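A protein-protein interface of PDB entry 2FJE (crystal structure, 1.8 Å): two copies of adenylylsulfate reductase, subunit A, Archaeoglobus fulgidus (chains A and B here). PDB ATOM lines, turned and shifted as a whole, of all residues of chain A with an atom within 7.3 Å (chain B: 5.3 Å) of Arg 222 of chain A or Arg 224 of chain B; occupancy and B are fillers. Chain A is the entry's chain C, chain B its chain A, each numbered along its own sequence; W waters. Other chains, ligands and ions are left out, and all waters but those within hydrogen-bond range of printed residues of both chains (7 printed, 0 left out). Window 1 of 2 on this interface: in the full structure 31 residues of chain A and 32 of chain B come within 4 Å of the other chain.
The backbone carbonyl oxygen of Arg 224 of chain A lies within hydrogen-bond range of the guanidinium group of Arg 222 of chain B (2.8 Å).
The guanidinium group (NH1) of Arg 222 of chain A sits at hydrogen-bond distance from the backbone carbonyl oxygen (O) of Arg 224 of chain B, 2.8 Å away.
The side-chain amino group (NZ) of Lys 523 of chain A sits at hydrogen-bond distance from the backbone carbonyl oxygen (O) of Arg 224 of chain B, 3.0 Å away.
The side-chain hydroxyl (OG) of Ser 225 of chain B is in hydrogen-bond range of the side-chain amino group (NZ) of Lys 523 of chain A, 3.0 Å away.
The side-chain carboxylate of Glu 527 of chain A sits close to the backbone carbonyl oxygen of Arg 224 of chain B (3.4 Å).
Of the 12 printed residues of chain B, 4 touch a printed residue of chain A.
Among the printed residues, 10 pairs touch across the chains.
Among the printed residues, no Asp or Glu carboxylate lies within 4 Å of a Lys or Arg side-chain nitrogen of the other chain.
The backbone carbonyl oxygen of Pro 389 of chain B sits at hydrogen-bond distance from the guanidinium group of Arg 224 of chain B, 2.6 Å away.
The side-chain hydroxyl (OH) of Tyr 536 of chain B is in hydrogen-bond range of the guanidinium group (NH2) of Arg 224 of chain B.
O of Gln 522 of chain A is in hydrogen-bond range of N of Arg 222 of chain A.
The guanidinium group (NE) of Arg 222 of chain A lies within salt-bridge range of the side-chain carboxylate (OD2) of Asp 526 of chain A.
The guanidinium group of Arg 222 of chain A is in salt-bridge range of the side-chain carboxylate of Glu 527 of chain A, at 3.4 Å.
NZ of Lys 523 of chain A is in salt-bridge range of OE2 of Glu 527 of chain A (2.7 Å).
Of the printed residues of chain B, Arg 224 of chain A touches Arg 222.
Of the printed residues of chain B, Ser 225 of chain A touches Arg 222.
Printed residues of chain B within 4 Å of Glu 527 of chain A: Arg 224 (3.4 Å).
Arg 224 of chain B touches three residues of chain A.
Ala 390 of chain B touches none of the printed residues of chain A.
The nearest residue of chain B that does not touch Arg 222 of chain A is Pro 223 of chain B (5.1 Å).
Arg 222 of chain A touches Arg 224 of chain B, and with the chains exchanged Arg 224 of chain A touches Arg 222 of chain B.
Arg 222 of chain A touches Ser 225 of chain B, and with the chains exchanged Ser 225 of chain A touches Arg 222 of chain B.
Arg 222 of chain A touches Thr 226 of chain B, and with the chains exchanged Thr 226 of chain A touches Arg 222 of chain B.
Thr 226 of chain A touches its own counterpart, Thr 226 of chain B.
Positions printed for both chains: 222, 223, 224, 225, 226, 390, 391 and 532.
Among the printed residues, merely in contact across the chains: Arg 222 of chain A with Ser 225 of chain B (3.8 Å), Arg 222 of chain A with Thr 226 of chain B (3.8 Å), Ser 225 of chain A with Arg 222 of chain B (3.8 Å), Thr 226 of chain A with Arg 222 of chain B (3.6 Å) and Thr 226 of chain A with Thr 226 of chain B (3.5 Å).
Water W1 lies within hydrogen-bond range of O of Pro 223 of chain B (2.7 Å) and NH1 of Arg 222 of chain A (3.3 Å).
Water W2 lies within hydrogen-bond range of O of Ala 533 of chain A (2.8 Å), O of Ile 532 of chain B (3.0 Å) and NH1 of Arg 224 of chain B (3.2 Å).
Water W7 lies within hydrogen-bond range of the backbone carbonyl oxygen of Thr 226 of chain B and the backbone carbonyl oxygen of Thr 226 of chain A.
Water W3 bridges N of Thr 226 of chain A (2.9 Å) and NH1 of Arg 222 of chain B (3.1 Å).
Water W4 bridges the guanidinium group of Arg 224 of chain B and the side-chain carboxylate of Glu 527 of chain A.
Water W6 bridges the backbone NH (N) of Thr 226 of chain B and the guanidinium group (NH1) of Arg 222 of chain A.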
ATOM      1  N   LEU A 219     -27.127 -12.338   6.945  1.00  0.00           N
ATOM      2  CA  LEU A 219     -25.758 -12.781   7.191  1.00  0.00           C
ATOM      3  C   LEU A 219     -25.315 -13.954   6.316  1.00  0.00           C
ATOM      4  O   LEU A 219     -24.366 -14.670   6.647  1.00  0.00           O
ATOM      5  CB  LEU A 219     -25.535 -13.094   8.679  1.00  0.00           C
ATOM      6  CG  LEU A 219     -25.465 -11.845   9.571  1.00  0.00           C
ATOM      7  CD1 LEU A 219     -25.133 -12.242  11.006  1.00  0.00           C
ATOM      8  CD2 LEU A 219     -24.399 -10.893   9.042  1.00  0.00           C
ATOM      9  N   LEU A 220     -26.005 -14.155   5.195  1.00  0.00           N
ATOM     10  CA  LEU A 220     -25.614 -15.205   4.260  1.00  0.00           C
ATOM     11  C   LEU A 220     -24.442 -14.623   3.481  1.00  0.00           C
ATOM     12  O   LEU A 220     -23.490 -15.330   3.135  1.00  0.00           O
ATOM     13  CB  LEU A 220     -26.745 -15.536   3.280  1.00  0.00           C
ATOM     14  CG  LEU A 220     -27.721 -16.651   3.659  1.00  0.00           C
ATOM     15  CD1 LEU A 220     -28.567 -16.229   4.842  1.00  0.00           C
ATOM     16  CD2 LEU A 220     -28.596 -16.967   2.458  1.00  0.00           C
ATOM     17  N   PHE A 221     -24.528 -13.319   3.221  1.00  0.00           N
ATOM     18  CA  PHE A 221     -23.500 -12.587   2.488  1.00  0.00           C
ATOM     19  C   PHE A 221     -22.639 -11.715   3.384  1.00  0.00           C
ATOM     20  O   PHE A 221     -23.118 -11.152   4.369  1.00  0.00           O
ATOM     21  CB  PHE A 221     -24.128 -11.675   1.427  1.00  0.00           C
ATOM     22  CG  PHE A 221     -24.743 -12.408   0.277  1.00  0.00           C
ATOM     23  CD1 PHE A 221     -25.993 -13.001   0.396  1.00  0.00           C
ATOM     24  CD2 PHE A 221     -24.062 -12.512  -0.932  1.00  0.00           C
ATOM     25  CE1 PHE A 221     -26.560 -13.690  -0.674  1.00  0.00           C
ATOM     26  CE2 PHE A 221     -24.618 -13.196  -2.006  1.00  0.00           C
ATOM     27  CZ  PHE A 221     -25.869 -13.786  -1.878  1.00  0.00           C
ATOM     28  N   ARG A 222     -21.367 -11.588   3.024  1.00  0.00           N
ATOM     29  CA  ARG A 222     -20.447 -10.744   3.778  1.00  0.00           C
ATOM     30  C   ARG A 222     -20.967  -9.305   3.709  1.00  0.00           C
ATOM     31  O   ARG A 222     -21.308  -8.816   2.634  1.00  0.00           O
ATOM     32  CB  ARG A 222     -19.044 -10.829   3.164  1.00  0.00           C
ATOM     33  CG  ARG A 222     -18.022  -9.883   3.786  1.00  0.00           C
ATOM     34  CD  ARG A 222     -16.601 -10.397   3.587  1.00  0.00           C
ATOM     35  NE  ARG A 222     -16.303 -10.684   2.189  1.00  0.00           N
ATOM     36  CZ  ARG A 222     -15.224 -11.342   1.776  1.00  0.00           C
ATOM     37  NH1 ARG A 222     -14.335 -11.781   2.655  1.00  0.00           N
ATOM     38  NH2 ARG A 222     -15.039 -11.569   0.485  1.00  0.00           N
ATOM     39  N   PRO A 223     -21.053  -8.617   4.861  1.00  0.00           N
ATOM     40  CA  PRO A 223     -21.539  -7.230   4.894  1.00  0.00           C
ATOM     41  C   PRO A 223     -20.462  -6.228   4.488  1.00  0.00           C
ATOM     42  O   PRO A 223     -19.295  -6.593   4.315  1.00  0.00           O
ATOM     43  CB  PRO A 223     -21.951  -7.034   6.359  1.00  0.00           C
ATOM     44  CG  PRO A 223     -22.115  -8.444   6.892  1.00  0.00           C
ATOM     45  CD  PRO A 223     -20.987  -9.172   6.221  1.00  0.00           C
ATOM     46  N   ARG A 224     -20.850  -4.962   4.352  1.00  0.00           N
ATOM     47  CA  ARG A 224     -19.895  -3.922   3.989  1.00  0.00           C
ATOM     48  C   ARG A 224     -19.046  -3.519   5.190  1.00  0.00           C
ATOM     49  O   ARG A 224     -18.110  -2.738   5.066  1.00  0.00           O
ATOM     50  CB  ARG A 224     -20.616  -2.710   3.399  1.00  0.00           C
ATOM     51  CG  ARG A 224     -21.191  -2.995   2.021  1.00  0.00           C
ATOM     52  CD  ARG A 224     -21.684  -1.741   1.335  1.00  0.00           C
ATOM     53  NE  ARG A 224     -22.166  -2.023  -0.016  1.00  0.00           N
ATOM     54  CZ  ARG A 224     -21.385  -2.293  -1.055  1.00  0.00           C
ATOM     55  NH1 ARG A 224     -20.065  -2.318  -0.911  1.00  0.00           N
ATOM     56  NH2 ARG A 224     -21.924  -2.534  -2.246  1.00  0.00           N
ATOM     57  N   SER A 225     -19.396  -4.056   6.356  1.00  0.00           N
ATOM     58  CA  SER A 225     -18.640  -3.830   7.585  1.00  0.00           C
ATOM     59  C   SER A 225     -18.410  -5.238   8.124  1.00  0.00           C
ATOM     60  O   SER A 225     -19.355  -6.016   8.287  1.00  0.00           O
ATOM     61  CB  SER A 225     -19.432  -2.972   8.573  1.00  0.00           C
ATOM     62  OG  SER A 225     -19.537  -1.640   8.091  1.00  0.00           O
ATOM     63  N   THR A 226     -17.152  -5.569   8.390  1.00  0.00           N
ATOM     64  CA  THR A 226     -16.803  -6.915   8.831  1.00  0.00           C
ATOM     65  C   THR A 226     -16.301  -7.119  10.259  1.00  0.00           C
ATOM     66  O   THR A 226     -15.922  -8.234  10.626  1.00  0.00           O
ATOM     67  CB  THR A 226     -15.772  -7.507   7.864  1.00  0.00           C
ATOM     68  OG1 THR A 226     -14.716  -6.558   7.666  1.00  0.00           O
ATOM     69  CG2 THR A 226     -16.421  -7.801   6.519  1.00  0.00           C
ATOM     70  N   ALA A 390     -26.646  -2.101   0.508  1.00  0.00           N
ATOM     71  CA  ALA A 390     -26.032  -3.078   1.399  1.00  0.00           C
ATOM     72  C   ALA A 390     -25.873  -4.406   0.667  1.00  0.00           C
ATOM     73  O   ALA A 390     -26.159  -4.502  -0.525  1.00  0.00           O
ATOM     74  CB  ALA A 390     -26.897  -3.270   2.637  1.00  0.00           C
ATOM     75  N   GLU A 391     -25.404  -5.425   1.381  1.00  0.00           N
ATOM     76  CA  GLU A 391     -25.244  -6.748   0.789  1.00  0.00           C
ATOM     77  C   GLU A 391     -26.646  -7.364   0.641  1.00  0.00           C
ATOM     78  O   GLU A 391     -27.620  -6.852   1.202  1.00  0.00           O
ATOM     79  CB  GLU A 391     -24.345  -7.637   1.669  1.00  0.00           C
ATOM     80  CG  GLU A 391     -24.977  -8.155   2.957  1.00  0.00           C
ATOM     81  CD  GLU A 391     -24.990  -7.130   4.084  1.00  0.00           C
ATOM     82  OE1 GLU A 391     -24.612  -5.962   3.852  1.00  0.00           O
ATOM     83  OE2 GLU A 391     -25.384  -7.503   5.210  1.00  0.00           O
ATOM     84  N   PRO A 392     -26.769  -8.463  -0.123  1.00  0.00           N
ATOM     85  CA  PRO A 392     -28.059  -9.130  -0.341  1.00  0.00           C
ATOM     86  C   PRO A 392     -28.708  -9.783   0.875  1.00  0.00           C
ATOM     87  O   PRO A 392     -28.024 -10.318   1.747  1.00  0.00           O
ATOM     88  CB  PRO A 392     -27.741 -10.186  -1.405  1.00  0.00           C
ATOM     89  CG  PRO A 392     -26.520  -9.663  -2.091  1.00  0.00           C
ATOM     90  CD  PRO A 392     -25.719  -9.079  -0.951  1.00  0.00           C
ATOM     91  N   LEU A 518     -19.535 -19.437   9.504  1.00  0.00           N
ATOM     92  CA  LEU A 518     -20.287 -18.304   8.965  1.00  0.00           C
ATOM     93  C   LEU A 518     -19.405 -17.361   8.148  1.00  0.00           C
ATOM     94  O   LEU A 518     -19.836 -16.833   7.124  1.00  0.00           O
ATOM     95  CB  LEU A 518     -20.983 -17.529  10.093  1.00  0.00           C
ATOM     96  CG  LEU A 518     -21.960 -16.428   9.657  1.00  0.00           C
ATOM     97  CD1 LEU A 518     -22.983 -17.003   8.677  1.00  0.00           C
ATOM     98  CD2 LEU A 518     -22.668 -15.841  10.880  1.00  0.00           C
ATOM     99  N   VAL A 519     -18.177 -17.142   8.607  1.00  0.00           N
ATOM    100  CA  VAL A 519     -17.239 -16.282   7.887  1.00  0.00           C
ATOM    101  C   VAL A 519     -17.015 -16.896   6.511  1.00  0.00           C
ATOM    102  O   VAL A 519     -16.982 -16.198   5.493  1.00  0.00           O
ATOM    103  CB  VAL A 519     -15.876 -16.200   8.631  1.00  0.00           C
ATOM    104  CG1 VAL A 519     -14.792 -15.655   7.701  1.00  0.00           C
ATOM    105  CG2 VAL A 519     -16.007 -15.307   9.850  1.00  0.00           C
ATOM    106  N   LEU A 521     -19.035 -19.051   4.879  1.00  0.00           N
ATOM    107  CA  LEU A 521     -20.248 -18.951   4.076  1.00  0.00           C
ATOM    108  C   LEU A 521     -20.347 -17.567   3.447  1.00  0.00           C
ATOM    109  O   LEU A 521     -20.613 -17.430   2.254  1.00  0.00           O
ATOM    110  CB  LEU A 521     -21.492 -19.178   4.938  1.00  0.00           C
ATOM    111  CG  LEU A 521     -22.808 -18.921   4.189  1.00  0.00           C
ATOM    112  CD1 LEU A 521     -22.935 -19.927   3.050  1.00  0.00           C
ATOM    113  CD2 LEU A 521     -24.000 -19.027   5.139  1.00  0.00           C
ATOM    114  N   GLN A 522     -20.135 -16.542   4.263  1.00  0.00           N
ATOM    115  CA  GLN A 522     -20.224 -15.166   3.786  1.00  0.00           C
ATOM    116  C   GLN A 522     -19.238 -14.848   2.671  1.00  0.00           C
ATOM    117  O   GLN A 522     -19.561 -14.113   1.737  1.00  0.00           O
ATOM    118  CB  GLN A 522     -20.038 -14.205   4.959  1.00  0.00           C
ATOM    119  CG  GLN A 522     -21.235 -14.205   5.906  1.00  0.00           C
ATOM    120  CD  GLN A 522     -21.010 -13.354   7.138  1.00  0.00           C
ATOM    121  OE1 GLN A 522     -19.955 -12.741   7.297  1.00  0.00           O
ATOM    122  NE2 GLN A 522     -22.003 -13.314   8.020  1.00  0.00           N
ATOM    123  N   LYS A 523     -18.040 -15.412   2.763  1.00  0.00           N
ATOM    124  CA  LYS A 523     -17.017 -15.184   1.746  1.00  0.00           C
ATOM    125  C   LYS A 523     -17.411 -15.861   0.431  1.00  0.00           C
ATOM    126  O   LYS A 523     -17.307 -15.265  -0.647  1.00  0.00           O
ATOM    127  CB  LYS A 523     -15.679 -15.715   2.251  1.00  0.00           C
ATOM    128  CG  LYS A 523     -14.501 -15.531   1.296  1.00  0.00           C
ATOM    129  CD  LYS A 523     -13.200 -15.936   1.976  1.00  0.00           C
ATOM    130  CE  LYS A 523     -12.055 -16.070   0.981  1.00  0.00           C
ATOM    131  NZ  LYS A 523     -11.751 -14.806   0.246  1.00  0.00           N
ATOM    132  N   ILE A 524     -17.872 -17.103   0.520  1.00  0.00           N
ATOM    133  CA  ILE A 524     -18.295 -17.842  -0.664  1.00  0.00           C
ATOM    134  C   ILE A 524     -19.403 -17.083  -1.388  1.00  0.00           C
ATOM    135  O   ILE A 524     -19.304 -16.808  -2.585  1.00  0.00           O
ATOM    136  CB  ILE A 524     -18.832 -19.247  -0.284  1.00  0.00           C
ATOM    137  CG1 ILE A 524     -17.697 -20.105   0.278  1.00  0.00           C
ATOM    138  CG2 ILE A 524     -19.459 -19.913  -1.502  1.00  0.00           C
ATOM    139  CD1 ILE A 524     -18.157 -21.432   0.843  1.00  0.00           C
ATOM    140  N   MET A 525     -20.455 -16.738  -0.654  1.00  0.00           N
ATOM    141  CA  MET A 525     -21.585 -16.033  -1.246  1.00  0.00           C
ATOM    142  C   MET A 525     -21.202 -14.665  -1.791  1.00  0.00           C
ATOM    143  O   MET A 525     -21.644 -14.270  -2.864  1.00  0.00           O
ATOM    144  CB  MET A 525     -22.712 -15.906  -0.220  1.00  0.00           C
ATOM    145  CG  MET A 525     -23.265 -17.260   0.229  1.00  0.00           C
ATOM    146  SD  MET A 525     -23.905 -18.240  -1.158  1.00  0.00           S
ATOM    147  CE  MET A 525     -25.452 -17.378  -1.466  1.00  0.00           C
ATOM    148  N   ASP A 526     -20.379 -13.940  -1.046  1.00  0.00           N
ATOM    149  CA  ASP A 526     -19.946 -12.619  -1.474  1.00  0.00           C
ATOM    150  C   ASP A 526     -19.167 -12.678  -2.786  1.00  0.00           C
ATOM    151  O   ASP A 526     -19.415 -11.896  -3.708  1.00  0.00           O
ATOM    152  CB  ASP A 526     -19.078 -11.989  -0.377  1.00  0.00           C
ATOM    153  CG  ASP A 526     -18.617 -10.587  -0.720  1.00  0.00           C
ATOM    154  OD1 ASP A 526     -19.388  -9.839  -1.357  1.00  0.00           O
ATOM    155  OD2 ASP A 526     -17.484 -10.230  -0.333  1.00  0.00           O
ATOM    156  N   GLU A 527     -18.242 -13.626  -2.884  1.00  0.00           N
ATOM    157  CA  GLU A 527     -17.403 -13.728  -4.071  1.00  0.00           C
ATOM    158  C   GLU A 527     -17.984 -14.448  -5.286  1.00  0.00           C
ATOM    159  O   GLU A 527     -17.585 -14.160  -6.417  1.00  0.00           O
ATOM    160  CB  GLU A 527     -16.058 -14.360  -3.680  1.00  0.00           C
ATOM    161  CG  GLU A 527     -15.365 -13.615  -2.538  1.00  0.00           C
ATOM    162  CD  GLU A 527     -14.042 -14.243  -2.115  1.00  0.00           C
ATOM    163  OE1 GLU A 527     -13.882 -15.475  -2.265  1.00  0.00           O
ATOM    164  OE2 GLU A 527     -13.171 -13.501  -1.612  1.00  0.00           O
ATOM    165  N   GLY A 531     -22.505 -10.962  -4.678  1.00  0.00           N
ATOM    166  CA  GLY A 531     -22.458 -10.207  -3.438  1.00  0.00           C
ATOM    167  C   GLY A 531     -21.841  -8.850  -3.737  1.00  0.00           C
ATOM    168  O   GLY A 531     -21.636  -8.510  -4.904  1.00  0.00           O
ATOM    169  N   ILE A 532     -21.533  -8.076  -2.700  1.00  0.00           N
ATOM    170  CA  ILE A 532     -20.949  -6.750  -2.898  1.00  0.00           C
ATOM    171  C   ILE A 532     -19.560  -6.781  -3.535  1.00  0.00           C
ATOM    172  O   ILE A 532     -19.157  -5.820  -4.188  1.00  0.00           O
ATOM    173  CB  ILE A 532     -20.841  -5.974  -1.569  1.00  0.00           C
ATOM    174  CG1 ILE A 532     -19.831  -6.657  -0.642  1.00  0.00           C
ATOM    175  CG2 ILE A 532     -22.208  -5.884  -0.906  1.00  0.00           C
ATOM    176  CD1 ILE A 532     -19.662  -5.961   0.697  1.00  0.00           C
ATOM    177  N   ALA A 533     -18.837  -7.884  -3.353  1.00  0.00           N
ATOM    178  CA  ALA A 533     -17.483  -8.016  -3.895  1.00  0.00           C
ATOM    179  C   ALA A 533     -17.401  -7.817  -5.405  1.00  0.00           C
ATOM    180  O   ALA A 533     -16.399  -7.321  -5.923  1.00  0.00           O
ATOM    181  CB  ALA A 533     -16.903  -9.381  -3.524  1.00  0.00           C
ATOM    182  N   THR A 534     -18.459  -8.199  -6.108  1.00  0.00           N
ATOM    183  CA  THR A 534     -18.495  -8.079  -7.561  1.00  0.00           C
ATOM    184  C   THR A 534     -19.614  -7.146  -8.018  1.00  0.00           C
ATOM    185  O   THR A 534     -20.105  -7.243  -9.142  1.00  0.00           O
ATOM    186  CB  THR A 534     -18.711  -9.455  -8.196  1.00  0.00           C
ATOM    187  OG1 THR A 534     -19.955 -10.000  -7.732  1.00  0.00           O
ATOM    188  CG2 THR A 534     -17.579 -10.399  -7.802  1.00  0.00           C
ATOM    189  N   ARG B 222      -8.601  -3.295   3.795  1.00  0.00           N
ATOM    190  CA  ARG B 222      -9.357  -4.490   4.144  1.00  0.00           C
ATOM    191  C   ARG B 222      -8.985  -5.588   3.148  1.00  0.00           C
ATOM    192  O   ARG B 222      -8.967  -5.352   1.938  1.00  0.00           O
ATOM    193  CB  ARG B 222     -10.862  -4.201   4.064  1.00  0.00           C
ATOM    194  CG  ARG B 222     -11.747  -5.419   4.278  1.00  0.00           C
ATOM    195  CD  ARG B 222     -13.120  -5.015   4.803  1.00  0.00           C
ATOM    196  NE  ARG B 222     -13.747  -3.992   3.973  1.00  0.00           N
ATOM    197  CZ  ARG B 222     -14.848  -3.328   4.311  1.00  0.00           C
ATOM    198  NH1 ARG B 222     -15.448  -3.577   5.467  1.00  0.00           N
ATOM    199  NH2 ARG B 222     -15.344  -2.408   3.497  1.00  0.00           N
ATOM    200  N   PRO B 223      -8.659  -6.796   3.641  1.00  0.00           N
ATOM    201  CA  PRO B 223      -8.289  -7.910   2.757  1.00  0.00           C
ATOM    202  C   PRO B 223      -9.516  -8.588   2.150  1.00  0.00           C
ATOM    203  O   PRO B 223     -10.655  -8.257   2.493  1.00  0.00           O
ATOM    204  CB  PRO B 223      -7.527  -8.866   3.686  1.00  0.00           C
ATOM    205  CG  PRO B 223      -7.122  -7.999   4.859  1.00  0.00           C
ATOM    206  CD  PRO B 223      -8.325  -7.117   5.037  1.00  0.00           C
ATOM    207  N   ARG B 224      -9.286  -9.544   1.255  1.00  0.00           N
ATOM    208  CA  ARG B 224     -10.391 -10.259   0.628  1.00  0.00           C
ATOM    209  C   ARG B 224     -10.946 -11.336   1.548  1.00  0.00           C
ATOM    210  O   ARG B 224     -11.938 -11.992   1.234  1.00  0.00           O
ATOM    211  CB  ARG B 224      -9.957 -10.859  -0.707  1.00  0.00           C
ATOM    212  CG  ARG B 224      -9.753  -9.798  -1.782  1.00  0.00           C
ATOM    213  CD  ARG B 224      -9.612 -10.396  -3.162  1.00  0.00           C
ATOM    214  NE  ARG B 224      -9.440  -9.361  -4.178  1.00  0.00           N
ATOM    215  CZ  ARG B 224     -10.422  -8.611  -4.670  1.00  0.00           C
ATOM    216  NH1 ARG B 224     -11.672  -8.771  -4.250  1.00  0.00           N
ATOM    217  NH2 ARG B 224     -10.150  -7.687  -5.584  1.00  0.00           N
ATOM    218  N   SER B 225     -10.283 -11.517   2.685  1.00  0.00           N
ATOM    219  CA  SER B 225     -10.710 -12.470   3.702  1.00  0.00           C
ATOM    220  C   SER B 225     -10.632 -11.655   4.985  1.00  0.00           C
ATOM    221  O   SER B 225      -9.594 -11.074   5.292  1.00  0.00           O
ATOM    222  CB  SER B 225      -9.770 -13.673   3.755  1.00  0.00           C
ATOM    223  OG  SER B 225      -9.889 -14.463   2.581  1.00  0.00           O
ATOM    224  N   THR B 226     -11.730 -11.609   5.732  1.00  0.00           N
ATOM    225  CA  THR B 226     -11.787 -10.793   6.935  1.00  0.00           C
ATOM    226  C   THR B 226     -11.885 -11.502   8.278  1.00  0.00           C
ATOM    227  O   THR B 226     -12.001 -10.845   9.314  1.00  0.00           O
ATOM    228  CB  THR B 226     -12.951  -9.802   6.825  1.00  0.00           C
ATOM    229  OG1 THR B 226     -14.157 -10.524   6.550  1.00  0.00           O
ATOM    230  CG2 THR B 226     -12.702  -8.818   5.692  1.00  0.00           C
ATOM    231  N   TYR B 270      -2.733 -16.759  -2.052  1.00  0.00           N
ATOM    232  CA  TYR B 270      -1.787 -15.833  -2.664  1.00  0.00           C
ATOM    233  C   TYR B 270      -0.433 -16.455  -2.965  1.00  0.00           C
ATOM    234  O   TYR B 270       0.607 -15.811  -2.826  1.00  0.00           O
ATOM    235  CB  TYR B 270      -1.631 -14.585  -1.790  1.00  0.00           C
ATOM    236  CG  TYR B 270      -2.926 -13.808  -1.664  1.00  0.00           C
ATOM    237  CD1 TYR B 270      -3.358 -13.322  -0.432  1.00  0.00           C
ATOM    238  CD2 TYR B 270      -3.738 -13.590  -2.779  1.00  0.00           C
ATOM    239  CE1 TYR B 270      -4.570 -12.644  -0.311  1.00  0.00           C
ATOM    240  CE2 TYR B 270      -4.946 -12.912  -2.670  1.00  0.00           C
ATOM    241  CZ  TYR B 270      -5.358 -12.445  -1.436  1.00  0.00           C
ATOM    242  OH  TYR B 270      -6.565 -11.796  -1.326  1.00  0.00           O
ATOM    243  N   ALA B 388      -6.433 -14.210  -8.416  1.00  0.00           N
ATOM    244  CA  ALA B 388      -7.106 -12.942  -8.202  1.00  0.00           C
ATOM    245  C   ALA B 388      -6.160 -11.912  -7.614  1.00  0.00           C
ATOM    246  O   ALA B 388      -5.145 -12.256  -7.002  1.00  0.00           O
ATOM    247  CB  ALA B 388      -8.295 -13.134  -7.271  1.00  0.00           C
ATOM    248  N   PRO B 389      -6.479 -10.626  -7.799  1.00  0.00           N
ATOM    249  CA  PRO B 389      -5.638  -9.554  -7.265  1.00  0.00           C
ATOM    250  C   PRO B 389      -6.005  -9.332  -5.798  1.00  0.00           C
ATOM    251  O   PRO B 389      -7.183  -9.317  -5.447  1.00  0.00           O
ATOM    252  CB  PRO B 389      -6.010  -8.368  -8.144  1.00  0.00           C
ATOM    253  CG  PRO B 389      -7.474  -8.587  -8.367  1.00  0.00           C
ATOM    254  CD  PRO B 389      -7.567 -10.079  -8.632  1.00  0.00           C
ATOM    255  N   ALA B 390      -5.000  -9.176  -4.943  1.00  0.00           N
ATOM    256  CA  ALA B 390      -5.242  -8.952  -3.521  1.00  0.00           C
ATOM    257  C   ALA B 390      -5.485  -7.471  -3.278  1.00  0.00           C
ATOM    258  O   ALA B 390      -5.525  -6.681  -4.222  1.00  0.00           O
ATOM    259  CB  ALA B 390      -4.045  -9.413  -2.714  1.00  0.00           C
ATOM    260  N   GLU B 391      -5.661  -7.091  -2.014  1.00  0.00           N
ATOM    261  CA  GLU B 391      -5.862  -5.687  -1.690  1.00  0.00           C
ATOM    262  C   GLU B 391      -4.508  -4.978  -1.838  1.00  0.00           C
ATOM    263  O   GLU B 391      -3.465  -5.630  -1.969  1.00  0.00           O
ATOM    264  CB  GLU B 391      -6.426  -5.521  -0.262  1.00  0.00           C
ATOM    265  CG  GLU B 391      -5.437  -5.749   0.884  1.00  0.00           C
ATOM    266  CD  GLU B 391      -5.180  -7.220   1.185  1.00  0.00           C
ATOM    267  OE1 GLU B 391      -5.676  -8.088   0.438  1.00  0.00           O
ATOM    268  OE2 GLU B 391      -4.476  -7.507   2.178  1.00  0.00           O
ATOM    269  N   ILE B 532     -10.236  -2.905  -2.659  1.00  0.00           N
ATOM    270  CA  ILE B 532     -10.963  -3.915  -3.414  1.00  0.00           C
ATOM    271  C   ILE B 532     -12.451  -3.590  -3.542  1.00  0.00           C
ATOM    272  O   ILE B 532     -13.090  -3.968  -4.522  1.00  0.00           O
ATOM    273  CB  ILE B 532     -10.810  -5.308  -2.767  1.00  0.00           C
ATOM    274  CG1 ILE B 532     -11.406  -5.306  -1.357  1.00  0.00           C
ATOM    275  CG2 ILE B 532      -9.330  -5.697  -2.718  1.00  0.00           C
ATOM    276  CD1 ILE B 532     -11.365  -6.665  -0.685  1.00  0.00           C
ATOM    277  N   TYR B 536     -10.446  -0.985  -7.012  1.00  0.00           N
ATOM    278  CA  TYR B 536      -9.325  -0.054  -7.054  1.00  0.00           C
ATOM    279  C   TYR B 536      -9.581   1.294  -7.715  1.00  0.00           C
ATOM    280  O   TYR B 536      -8.658   1.903  -8.256  1.00  0.00           O
ATOM    281  CB  TYR B 536      -8.128  -0.732  -7.722  1.00  0.00           C
ATOM    282  CG  TYR B 536      -7.935  -2.163  -7.271  1.00  0.00           C
ATOM    283  CD1 TYR B 536      -8.407  -3.227  -8.038  1.00  0.00           C
ATOM    284  CD2 TYR B 536      -7.322  -2.450  -6.053  1.00  0.00           C
ATOM    285  CE1 TYR B 536      -8.273  -4.546  -7.602  1.00  0.00           C
ATOM    286  CE2 TYR B 536      -7.183  -3.763  -5.605  1.00  0.00           C
ATOM    287  CZ  TYR B 536      -7.662  -4.804  -6.383  1.00  0.00           C
ATOM    288  OH  TYR B 536      -7.534  -6.101  -5.941  1.00  0.00           O
HETATM  289  O   HOH W   1     -13.264  -8.777   2.028  1.00  0.00           O
HETATM  290  O   HOH W   2     -14.180  -6.762  -4.299  1.00  0.00           O
HETATM  291  O   HOH W   3     -15.543  -3.154   8.576  1.00  0.00           O
HETATM  292  O   HOH W   4     -13.193 -10.639  -2.606  1.00  0.00           O
HETATM  293  O   HOH W   5     -16.916  -5.685   3.428  1.00  0.00           O
HETATM  294  O   HOH W   6     -13.472 -13.850   4.872  1.00  0.00           O
HETATM  295  O   HOH W   7     -12.965  -8.432  10.582  1.00  0.00           O
